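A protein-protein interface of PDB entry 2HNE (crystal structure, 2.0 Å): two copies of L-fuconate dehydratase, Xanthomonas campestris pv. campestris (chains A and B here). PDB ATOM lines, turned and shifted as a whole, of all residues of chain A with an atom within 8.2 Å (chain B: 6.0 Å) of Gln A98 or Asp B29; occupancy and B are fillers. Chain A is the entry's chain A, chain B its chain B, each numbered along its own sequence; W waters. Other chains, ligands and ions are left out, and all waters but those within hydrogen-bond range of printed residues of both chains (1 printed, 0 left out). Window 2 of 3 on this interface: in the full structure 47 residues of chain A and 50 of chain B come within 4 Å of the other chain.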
ATOM      1  N   HIS A  73     -15.175  18.503  -0.924  1.00  0.00           N
ATOM      2  CA  HIS A  73     -14.110  17.710  -0.334  1.00  0.00           C
ATOM      3  C   HIS A  73     -12.854  18.520  -0.042  1.00  0.00           C
ATOM      4  O   HIS A  73     -12.066  18.146   0.814  1.00  0.00           O
ATOM      5  CB  HIS A  73     -13.707  16.568  -1.271  1.00  0.00           C
ATOM      6  CG  HIS A  73     -14.815  15.619  -1.590  1.00  0.00           C
ATOM      7  ND1 HIS A  73     -14.882  14.349  -1.059  1.00  0.00           N
ATOM      8  CD2 HIS A  73     -15.887  15.743  -2.406  1.00  0.00           C
ATOM      9  CE1 HIS A  73     -15.947  13.732  -1.537  1.00  0.00           C
ATOM     10  NE2 HIS A  73     -16.573  14.555  -2.357  1.00  0.00           N
ATOM     11  N   LEU A  93     -10.469  11.581  -1.594  1.00  0.00           N
ATOM     12  CA  LEU A  93     -11.220  11.662  -2.838  1.00  0.00           C
ATOM     13  C   LEU A  93     -11.505  10.281  -3.423  1.00  0.00           C
ATOM     14  O   LEU A  93     -12.644   9.955  -3.749  1.00  0.00           O
ATOM     15  CB  LEU A  93     -10.434  12.504  -3.856  1.00  0.00           C
ATOM     16  CG  LEU A  93     -10.671  14.014  -3.901  1.00  0.00           C
ATOM     17  CD1 LEU A  93     -11.174  14.517  -2.573  1.00  0.00           C
ATOM     18  CD2 LEU A  93      -9.376  14.714  -4.307  1.00  0.00           C
ATOM     19  N   THR A  94     -10.465   9.467  -3.541  1.00  0.00           N
ATOM     20  CA  THR A  94     -10.605   8.134  -4.110  1.00  0.00           C
ATOM     21  C   THR A  94     -11.430   7.181  -3.247  1.00  0.00           C
ATOM     22  O   THR A  94     -12.038   6.248  -3.774  1.00  0.00           O
ATOM     23  CB  THR A  94      -9.224   7.512  -4.376  1.00  0.00           C
ATOM     24  OG1 THR A  94      -8.460   8.411  -5.190  1.00  0.00           O
ATOM     25  CG2 THR A  94      -9.365   6.190  -5.123  1.00  0.00           C
ATOM     26  N   ASN A  95     -11.456   7.414  -1.935  1.00  0.00           N
ATOM     27  CA  ASN A  95     -12.225   6.561  -1.029  1.00  0.00           C
ATOM     28  C   ASN A  95     -13.685   6.948  -0.826  1.00  0.00           C
ATOM     29  O   ASN A  95     -14.379   6.302  -0.037  1.00  0.00           O
ATOM     30  CB  ASN A  95     -11.565   6.466   0.357  1.00  0.00           C
ATOM     31  CG  ASN A  95     -10.371   5.533   0.376  1.00  0.00           C
ATOM     32  OD1 ASN A  95     -10.276   4.601  -0.429  1.00  0.00           O
ATOM     33  ND2 ASN A  95      -9.453   5.766   1.317  1.00  0.00           N
ATOM     34  N   ASP A  96     -14.159   8.000  -1.492  1.00  0.00           N
ATOM     35  CA  ASP A  96     -15.570   8.378  -1.356  1.00  0.00           C
ATOM     36  C   ASP A  96     -16.342   7.308  -2.141  1.00  0.00           C
ATOM     37  O   ASP A  96     -16.349   7.318  -3.370  1.00  0.00           O
ATOM     38  CB  ASP A  96     -15.833   9.767  -1.956  1.00  0.00           C
ATOM     39  CG  ASP A  96     -17.297  10.193  -1.838  1.00  0.00           C
ATOM     40  OD1 ASP A  96     -18.182   9.314  -1.891  1.00  0.00           O
ATOM     41  OD2 ASP A  96     -17.570  11.404  -1.711  1.00  0.00           O
ATOM     42  N   SER A  97     -16.978   6.383  -1.426  1.00  0.00           N
ATOM     43  CA  SER A  97     -17.709   5.284  -2.055  1.00  0.00           C
ATOM     44  C   SER A  97     -18.754   5.716  -3.083  1.00  0.00           C
ATOM     45  O   SER A  97     -18.989   5.018  -4.069  1.00  0.00           O
ATOM     46  CB  SER A  97     -18.385   4.413  -0.988  1.00  0.00           C
ATOM     47  OG  SER A  97     -19.384   5.138  -0.291  1.00  0.00           O
ATOM     48  N   GLN A  98     -19.378   6.862  -2.850  1.00  0.00           N
ATOM     49  CA  GLN A  98     -20.405   7.340  -3.752  1.00  0.00           C
ATOM     50  C   GLN A  98     -19.794   7.807  -5.075  1.00  0.00           C
ATOM     51  O   GLN A  98     -20.338   7.536  -6.152  1.00  0.00           O
ATOM     52  CB  GLN A  98     -21.237   8.406  -3.028  1.00  0.00           C
ATOM     53  CG  GLN A  98     -22.116   7.715  -1.965  1.00  0.00           C
ATOM     54  CD  GLN A  98     -22.947   8.642  -1.106  1.00  0.00           C
ATOM     55  OE1 GLN A  98     -23.420   9.686  -1.559  1.00  0.00           O
ATOM     56  NE2 GLN A  98     -23.159   8.241   0.144  1.00  0.00           N
ATOM     57  N   LEU A  99     -18.649   8.476  -5.003  1.00  0.00           N
ATOM     58  CA  LEU A  99     -17.973   8.894  -6.220  1.00  0.00           C
ATOM     59  C   LEU A  99     -17.333   7.650  -6.862  1.00  0.00           C
ATOM     60  O   LEU A  99     -17.210   7.572  -8.084  1.00  0.00           O
ATOM     61  CB  LEU A  99     -16.926   9.960  -5.903  1.00  0.00           C
ATOM     62  CG  LEU A  99     -17.357  11.427  -6.066  1.00  0.00           C
ATOM     63  CD1 LEU A  99     -18.815  11.624  -5.730  1.00  0.00           C
ATOM     64  CD2 LEU A  99     -16.464  12.305  -5.209  1.00  0.00           C
ATOM     65  N   ARG A 100     -16.945   6.665  -6.049  1.00  0.00           N
ATOM     66  CA  ARG A 100     -16.361   5.438  -6.591  1.00  0.00           C
ATOM     67  C   ARG A 100     -17.357   4.730  -7.516  1.00  0.00           C
ATOM     68  O   ARG A 100     -16.964   4.098  -8.505  1.00  0.00           O
ATOM     69  CB  ARG A 100     -15.963   4.458  -5.480  1.00  0.00           C
ATOM     70  CG  ARG A 100     -14.745   4.834  -4.666  1.00  0.00           C
ATOM     71  CD  ARG A 100     -14.308   3.649  -3.804  1.00  0.00           C
ATOM     72  NE  ARG A 100     -13.739   2.557  -4.598  1.00  0.00           N
ATOM     73  CZ  ARG A 100     -12.500   2.548  -5.084  1.00  0.00           C
ATOM     74  NH1 ARG A 100     -11.689   3.572  -4.853  1.00  0.00           N
ATOM     75  NH2 ARG A 100     -12.073   1.520  -5.814  1.00  0.00           N
ATOM     76  N   TRP A 101     -18.646   4.828  -7.188  1.00  0.00           N
ATOM     77  CA  TRP A 101     -19.687   4.183  -7.991  1.00  0.00           C
ATOM     78  C   TRP A 101     -19.669   4.649  -9.459  1.00  0.00           C
ATOM     79  O   TRP A 101     -19.963   3.874 -10.373  1.00  0.00           O
ATOM     80  CB  TRP A 101     -21.066   4.454  -7.381  1.00  0.00           C
ATOM     81  CG  TRP A 101     -22.145   3.577  -7.947  1.00  0.00           C
ATOM     82  CD1 TRP A 101     -22.956   3.850  -9.016  1.00  0.00           C
ATOM     83  CD2 TRP A 101     -22.494   2.262  -7.504  1.00  0.00           C
ATOM     84  NE1 TRP A 101     -23.785   2.783  -9.264  1.00  0.00           N
ATOM     85  CE2 TRP A 101     -23.521   1.794  -8.352  1.00  0.00           C
ATOM     86  CE3 TRP A 101     -22.034   1.429  -6.471  1.00  0.00           C
ATOM     87  CZ2 TRP A 101     -24.101   0.527  -8.201  1.00  0.00           C
ATOM     88  CZ3 TRP A 101     -22.609   0.171  -6.322  1.00  0.00           C
ATOM     89  CH2 TRP A 101     -23.632  -0.267  -7.183  1.00  0.00           C
ATOM     90  N   LEU A 102     -19.327   5.913  -9.678  1.00  0.00           N
ATOM     91  CA  LEU A 102     -19.260   6.453 -11.039  1.00  0.00           C
ATOM     92  C   LEU A 102     -18.082   5.858 -11.822  1.00  0.00           C
ATOM     93  O   LEU A 102     -17.949   6.075 -13.027  1.00  0.00           O
ATOM     94  CB  LEU A 102     -19.144   7.979 -11.000  1.00  0.00           C
ATOM     95  CG  LEU A 102     -20.388   8.810 -10.626  1.00  0.00           C
ATOM     96  CD1 LEU A 102     -21.533   8.436 -11.539  1.00  0.00           C
ATOM     97  CD2 LEU A 102     -20.790   8.566  -9.186  1.00  0.00           C
ATOM     98  N   GLY A 103     -17.230   5.107 -11.133  1.00  0.00           N
ATOM     99  CA  GLY A 103     -16.097   4.476 -11.789  1.00  0.00           C
ATOM    100  C   GLY A 103     -16.203   2.963 -11.699  1.00  0.00           C
ATOM    101  O   GLY A 103     -16.986   2.354 -12.421  1.00  0.00           O
ATOM    102  N   MET A 109     -14.952  10.732 -13.792  1.00  0.00           N
ATOM    103  CA  MET A 109     -14.835  10.990 -12.363  1.00  0.00           C
ATOM    104  C   MET A 109     -13.410  10.783 -11.854  1.00  0.00           C
ATOM    105  O   MET A 109     -12.921  11.564 -11.059  1.00  0.00           O
ATOM    106  CB  MET A 109     -15.810  10.104 -11.584  1.00  0.00           C
ATOM    107  CG  MET A 109     -16.060  10.578 -10.168  1.00  0.00           C
ATOM    108  SD  MET A 109     -16.753  12.254 -10.110  1.00  0.00           S
ATOM    109  CE  MET A 109     -18.479  11.905  -9.921  1.00  0.00           C
ATOM    110  N   SER B  17     -30.402   5.845   2.929  1.00  0.00           N
ATOM    111  CA  SER B  17     -29.399   5.717   3.982  1.00  0.00           C
ATOM    112  C   SER B  17     -29.986   5.907   5.379  1.00  0.00           C
ATOM    113  O   SER B  17     -29.330   5.615   6.376  1.00  0.00           O
ATOM    114  CB  SER B  17     -28.268   6.721   3.759  1.00  0.00           C
ATOM    115  OG  SER B  17     -28.748   8.051   3.783  1.00  0.00           O
ATOM    116  N   LEU B  20     -30.219   2.454   6.352  1.00  0.00           N
ATOM    117  CA  LEU B  20     -29.044   1.663   6.010  1.00  0.00           C
ATOM    118  C   LEU B  20     -29.355   0.553   5.017  1.00  0.00           C
ATOM    119  O   LEU B  20     -28.646  -0.452   4.960  1.00  0.00           O
ATOM    120  CB  LEU B  20     -28.410   1.059   7.266  1.00  0.00           C
ATOM    121  CG  LEU B  20     -27.700   2.052   8.188  1.00  0.00           C
ATOM    122  CD1 LEU B  20     -27.054   1.301   9.343  1.00  0.00           C
ATOM    123  CD2 LEU B  20     -26.648   2.822   7.392  1.00  0.00           C
ATOM    124  N   SER B  23     -26.770  -0.988   2.501  1.00  0.00           N
ATOM    125  CA  SER B  23     -25.522  -0.929   3.252  1.00  0.00           C
ATOM    126  C   SER B  23     -24.595  -2.104   2.911  1.00  0.00           C
ATOM    127  O   SER B  23     -25.036  -3.253   2.877  1.00  0.00           O
ATOM    128  CB  SER B  23     -25.848  -0.957   4.749  1.00  0.00           C
ATOM    129  OG  SER B  23     -24.674  -1.065   5.526  1.00  0.00           O
ATOM    130  N   ASP B  24     -23.322  -1.821   2.644  1.00  0.00           N
ATOM    131  CA  ASP B  24     -22.365  -2.891   2.345  1.00  0.00           C
ATOM    132  C   ASP B  24     -20.926  -2.512   2.726  1.00  0.00           C
ATOM    133  O   ASP B  24     -20.665  -1.386   3.142  1.00  0.00           O
ATOM    134  CB  ASP B  24     -22.471  -3.340   0.867  1.00  0.00           C
ATOM    135  CG  ASP B  24     -21.923  -2.314  -0.122  1.00  0.00           C
ATOM    136  OD1 ASP B  24     -20.725  -1.969  -0.029  1.00  0.00           O
ATOM    137  OD2 ASP B  24     -22.694  -1.866  -1.005  1.00  0.00           O
ATOM    138  N   ASN B  27     -19.741   0.501   0.407  1.00  0.00           N
ATOM    139  CA  ASN B  27     -20.677   1.625   0.456  1.00  0.00           C
ATOM    140  C   ASN B  27     -21.519   1.524   1.731  1.00  0.00           C
ATOM    141  O   ASN B  27     -22.557   0.871   1.746  1.00  0.00           O
ATOM    142  CB  ASN B  27     -21.580   1.568  -0.771  1.00  0.00           C
ATOM    143  CG  ASN B  27     -20.799   1.281  -2.040  1.00  0.00           C
ATOM    144  OD1 ASN B  27     -19.900   2.042  -2.407  1.00  0.00           O
ATOM    145  ND2 ASN B  27     -21.123   0.177  -2.704  1.00  0.00           N
ATOM    146  N   PRO B  28     -21.086   2.187   2.810  1.00  0.00           N
ATOM    147  CA  PRO B  28     -21.790   2.166   4.097  1.00  0.00           C
ATOM    148  C   PRO B  28     -23.124   2.913   4.199  1.00  0.00           C
ATOM    149  O   PRO B  28     -23.977   2.549   5.012  1.00  0.00           O
ATOM    150  CB  PRO B  28     -20.749   2.735   5.051  1.00  0.00           C
ATOM    151  CG  PRO B  28     -20.099   3.795   4.193  1.00  0.00           C
ATOM    152  CD  PRO B  28     -19.904   3.069   2.873  1.00  0.00           C
ATOM    153  N   ASP B  29     -23.318   3.943   3.380  1.00  0.00           N
ATOM    154  CA  ASP B  29     -24.547   4.736   3.462  1.00  0.00           C
ATOM    155  C   ASP B  29     -25.067   5.221   2.109  1.00  0.00           C
ATOM    156  O   ASP B  29     -25.276   6.420   1.901  1.00  0.00           O
ATOM    157  CB  ASP B  29     -24.285   5.934   4.367  1.00  0.00           C
ATOM    158  CG  ASP B  29     -23.121   6.780   3.882  1.00  0.00           C
ATOM    159  OD1 ASP B  29     -22.170   6.216   3.292  1.00  0.00           O
ATOM    160  OD2 ASP B  29     -23.149   8.007   4.094  1.00  0.00           O
ATOM    161  N   PRO B  30     -25.317   4.290   1.180  1.00  0.00           N
ATOM    162  CA  PRO B  30     -25.811   4.684  -0.144  1.00  0.00           C
ATOM    163  C   PRO B  30     -27.195   5.310  -0.155  1.00  0.00           C
ATOM    164  O   PRO B  30     -28.102   4.870   0.557  1.00  0.00           O
ATOM    165  CB  PRO B  30     -25.779   3.376  -0.924  1.00  0.00           C
ATOM    166  CG  PRO B  30     -26.106   2.355   0.157  1.00  0.00           C
ATOM    167  CD  PRO B  30     -25.251   2.823   1.310  1.00  0.00           C
ATOM    168  N   ASP B  31     -27.333   6.359  -0.960  1.00  0.00           N
ATOM    169  CA  ASP B  31     -28.600   7.052  -1.148  1.00  0.00           C
ATOM    170  C   ASP B  31     -29.011   6.734  -2.578  1.00  0.00           C
ATOM    171  O   ASP B  31     -28.636   7.443  -3.512  1.00  0.00           O
ATOM    172  CB  ASP B  31     -28.415   8.550  -0.978  1.00  0.00           C
ATOM    173  CG  ASP B  31     -28.483   8.978   0.467  1.00  0.00           C
ATOM    174  OD1 ASP B  31     -27.821   9.977   0.817  1.00  0.00           O
ATOM    175  OD2 ASP B  31     -29.213   8.319   1.245  1.00  0.00           O
ATOM    176  N   THR B  55     -27.115   5.499  -9.578  1.00  0.00           N
ATOM    177  CA  THR B  55     -26.025   6.112  -8.820  1.00  0.00           C
ATOM    178  C   THR B  55     -26.369   5.907  -7.325  1.00  0.00           C
ATOM    179  O   THR B  55     -27.488   5.508  -7.010  1.00  0.00           O
ATOM    180  CB  THR B  55     -25.982   7.621  -9.178  1.00  0.00           C
ATOM    181  OG1 THR B  55     -25.191   7.800 -10.365  1.00  0.00           O
ATOM    182  CG2 THR B  55     -25.451   8.456  -8.056  1.00  0.00           C
ATOM    183  N   ILE B  56     -25.432   6.160  -6.412  1.00  0.00           N
ATOM    184  CA  ILE B  56     -25.748   6.001  -4.990  1.00  0.00           C
ATOM    185  C   ILE B  56     -25.610   7.281  -4.173  1.00  0.00           C
ATOM    186  O   ILE B  56     -25.243   7.238  -2.990  1.00  0.00           O
ATOM    187  CB  ILE B  56     -24.911   4.886  -4.309  1.00  0.00           C
ATOM    188  CG1 ILE B  56     -23.417   5.103  -4.544  1.00  0.00           C
ATOM    189  CG2 ILE B  56     -25.358   3.533  -4.817  1.00  0.00           C
ATOM    190  CD1 ILE B  56     -22.543   4.263  -3.630  1.00  0.00           C
ATOM    191  N   GLY B  57     -25.923   8.418  -4.797  1.00  0.00           N
ATOM    192  CA  GLY B  57     -25.849   9.689  -4.093  1.00  0.00           C
ATOM    193  C   GLY B  57     -24.987  10.746  -4.750  1.00  0.00           C
ATOM    194  O   GLY B  57     -25.294  11.197  -5.855  1.00  0.00           O
ATOM    195  N   ARG B  58     -23.919  11.156  -4.063  1.00  0.00           N
ATOM    196  CA  ARG B  58     -23.012  12.171  -4.592  1.00  0.00           C
ATOM    197  C   ARG B  58     -22.557  11.772  -5.985  1.00  0.00           C
ATOM    198  O   ARG B  58     -22.288  10.601  -6.242  1.00  0.00           O
ATOM    199  CB  ARG B  58     -21.776  12.316  -3.705  1.00  0.00           C
ATOM    200  CG  ARG B  58     -22.072  12.630  -2.263  1.00  0.00           C
ATOM    201  CD  ARG B  58     -20.831  12.478  -1.404  1.00  0.00           C
ATOM    202  NE  ARG B  58     -21.226  12.095  -0.054  1.00  0.00           N
ATOM    203  CZ  ARG B  58     -20.902  10.943   0.521  1.00  0.00           C
ATOM    204  NH1 ARG B  58     -20.159  10.056  -0.125  1.00  0.00           N
ATOM    205  NH2 ARG B  58     -21.359  10.663   1.733  1.00  0.00           N
ATOM    206  N   GLY B  59     -22.459  12.756  -6.874  1.00  0.00           N
ATOM    207  CA  GLY B  59     -22.029  12.478  -8.230  1.00  0.00           C
ATOM    208  C   GLY B  59     -23.188  12.204  -9.169  1.00  0.00           C
ATOM    209  O   GLY B  59     -23.005  12.110 -10.384  1.00  0.00           O
HETATM  210  O   HOH W   1     -22.966   7.648  -6.924  1.00  0.00           O
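The backbone carbonyl oxygen of Ile B56 sits close to the side-chain amide oxygen of Gln A98. OD1 of Asp A96 lies within salt-bridge range of NH1 of Arg B58, 2.8 Å away. The backbone NH (N) of Arg B58 lies within hydrogen-bond range of the side-chain amide oxygen (OE1) of Gln A98, 2.9 Å away. O of Asp B29 is in hydrogen-bond range of NE2 of Gln A98, 3.3 Å away.
Among the printed residues, merely in contact across the chains: Ser A97 with Asn B27, Ser A97 with Pro B28, Ser A97 with Ile B56, Gln A98 with Gly B57, Leu A99 with Arg B58, Leu A99 with Gly B59, Trp A101 with Asn B27, Trp A101 with Thr B55, Trp A101 with Ile B56, Leu A102 with Thr B55, Leu A102 with Arg B58 and Met A109 with Gly B59.
No position is printed for both chains. Of the 16 pairs that touch across the chains among the printed residues, none has its exchanged pair printed and touching as well.
Of chain B, only Asp B29, Ile B56, Gly B57 and Arg B58 come within 4 Å of Gln A98. Of chain A, only Gln A98 (3.3 Å) comes within 4 Å of Asp B29. Pro B28 touches just one residue of chain A: Ser A97 (3.8 Å). No residue of chain A comes within 4 Å of Pro B30. Of the printed residues of chain A, Gly B59 touches Leu A99 and Met A109. Printed residues of chain A within 4 Å of Arg B58: Asp A96 (2.8 Å), Gln A98 (2.9 Å), Leu A99 (3.7 Å) and Leu A102 (3.9 Å). Leu A93 touches none of the printed residues of chain B. Gly A103 touches none of the printed residues of chain B. The nearest residue of chain A that does not touch Asp B29 is Ser A97 (4.7 Å). The nearest printed residue of chain B that does not touch Asp A96 is Asn B27 (6.4 Å).
Water W1 lies within hydrogen-bond range of O of Gln A98, N of Ile B56 and O of Arg B58.
Of the 13 printed residues of chain A, 7 touch a printed residue of chain B. Printed residues of chain A that touch a printed residue of chain B: Asp A96, Ser A97, Gln A98, Leu A99, Trp A101, Leu A102 and Met A109. Hydrophobic or aromatic side chains of chain A that line the printed part of chain B: Leu A99, Trp A101, Leu A102 and Met A109. Hydrophobic or aromatic side chains of chain B within 4 Å of the printed part of chain A: Pro B28 and Ile B56. Among the printed residues, 16 pairs touch across the chains. Among the printed residues, Asp or Glu carboxylates within 4 Å of a Lys or Arg side-chain nitrogen of the other chain: Asp A96 with Arg B58.
The backbone NH (N) of Asp B31 is in hydrogen-bond range of the backbone carbonyl oxygen (O) of Ile B56, 3.0 Å away. The backbone NH of Gln A98 lies within hydrogen-bond range of the side-chain carboxylate of Asp A96, at 2.9 Å. A ring nitrogen (NE2) of His A73 lies close to the side-chain carboxylate (OD2) of Asp A96, at 3.4 Å. The side-chain carboxylate of Asp B24 is in hydrogen-bond range of the backbone NH of Asn B27, 2.7 Å away. The guanidinium group of Arg B58 is in salt-bridge range of the side-chain carboxylate of Asp B29 (3.98 Å). OD1 of Asp A96 lies within hydrogen-bond range of N of Leu A99 (3.3 Å).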
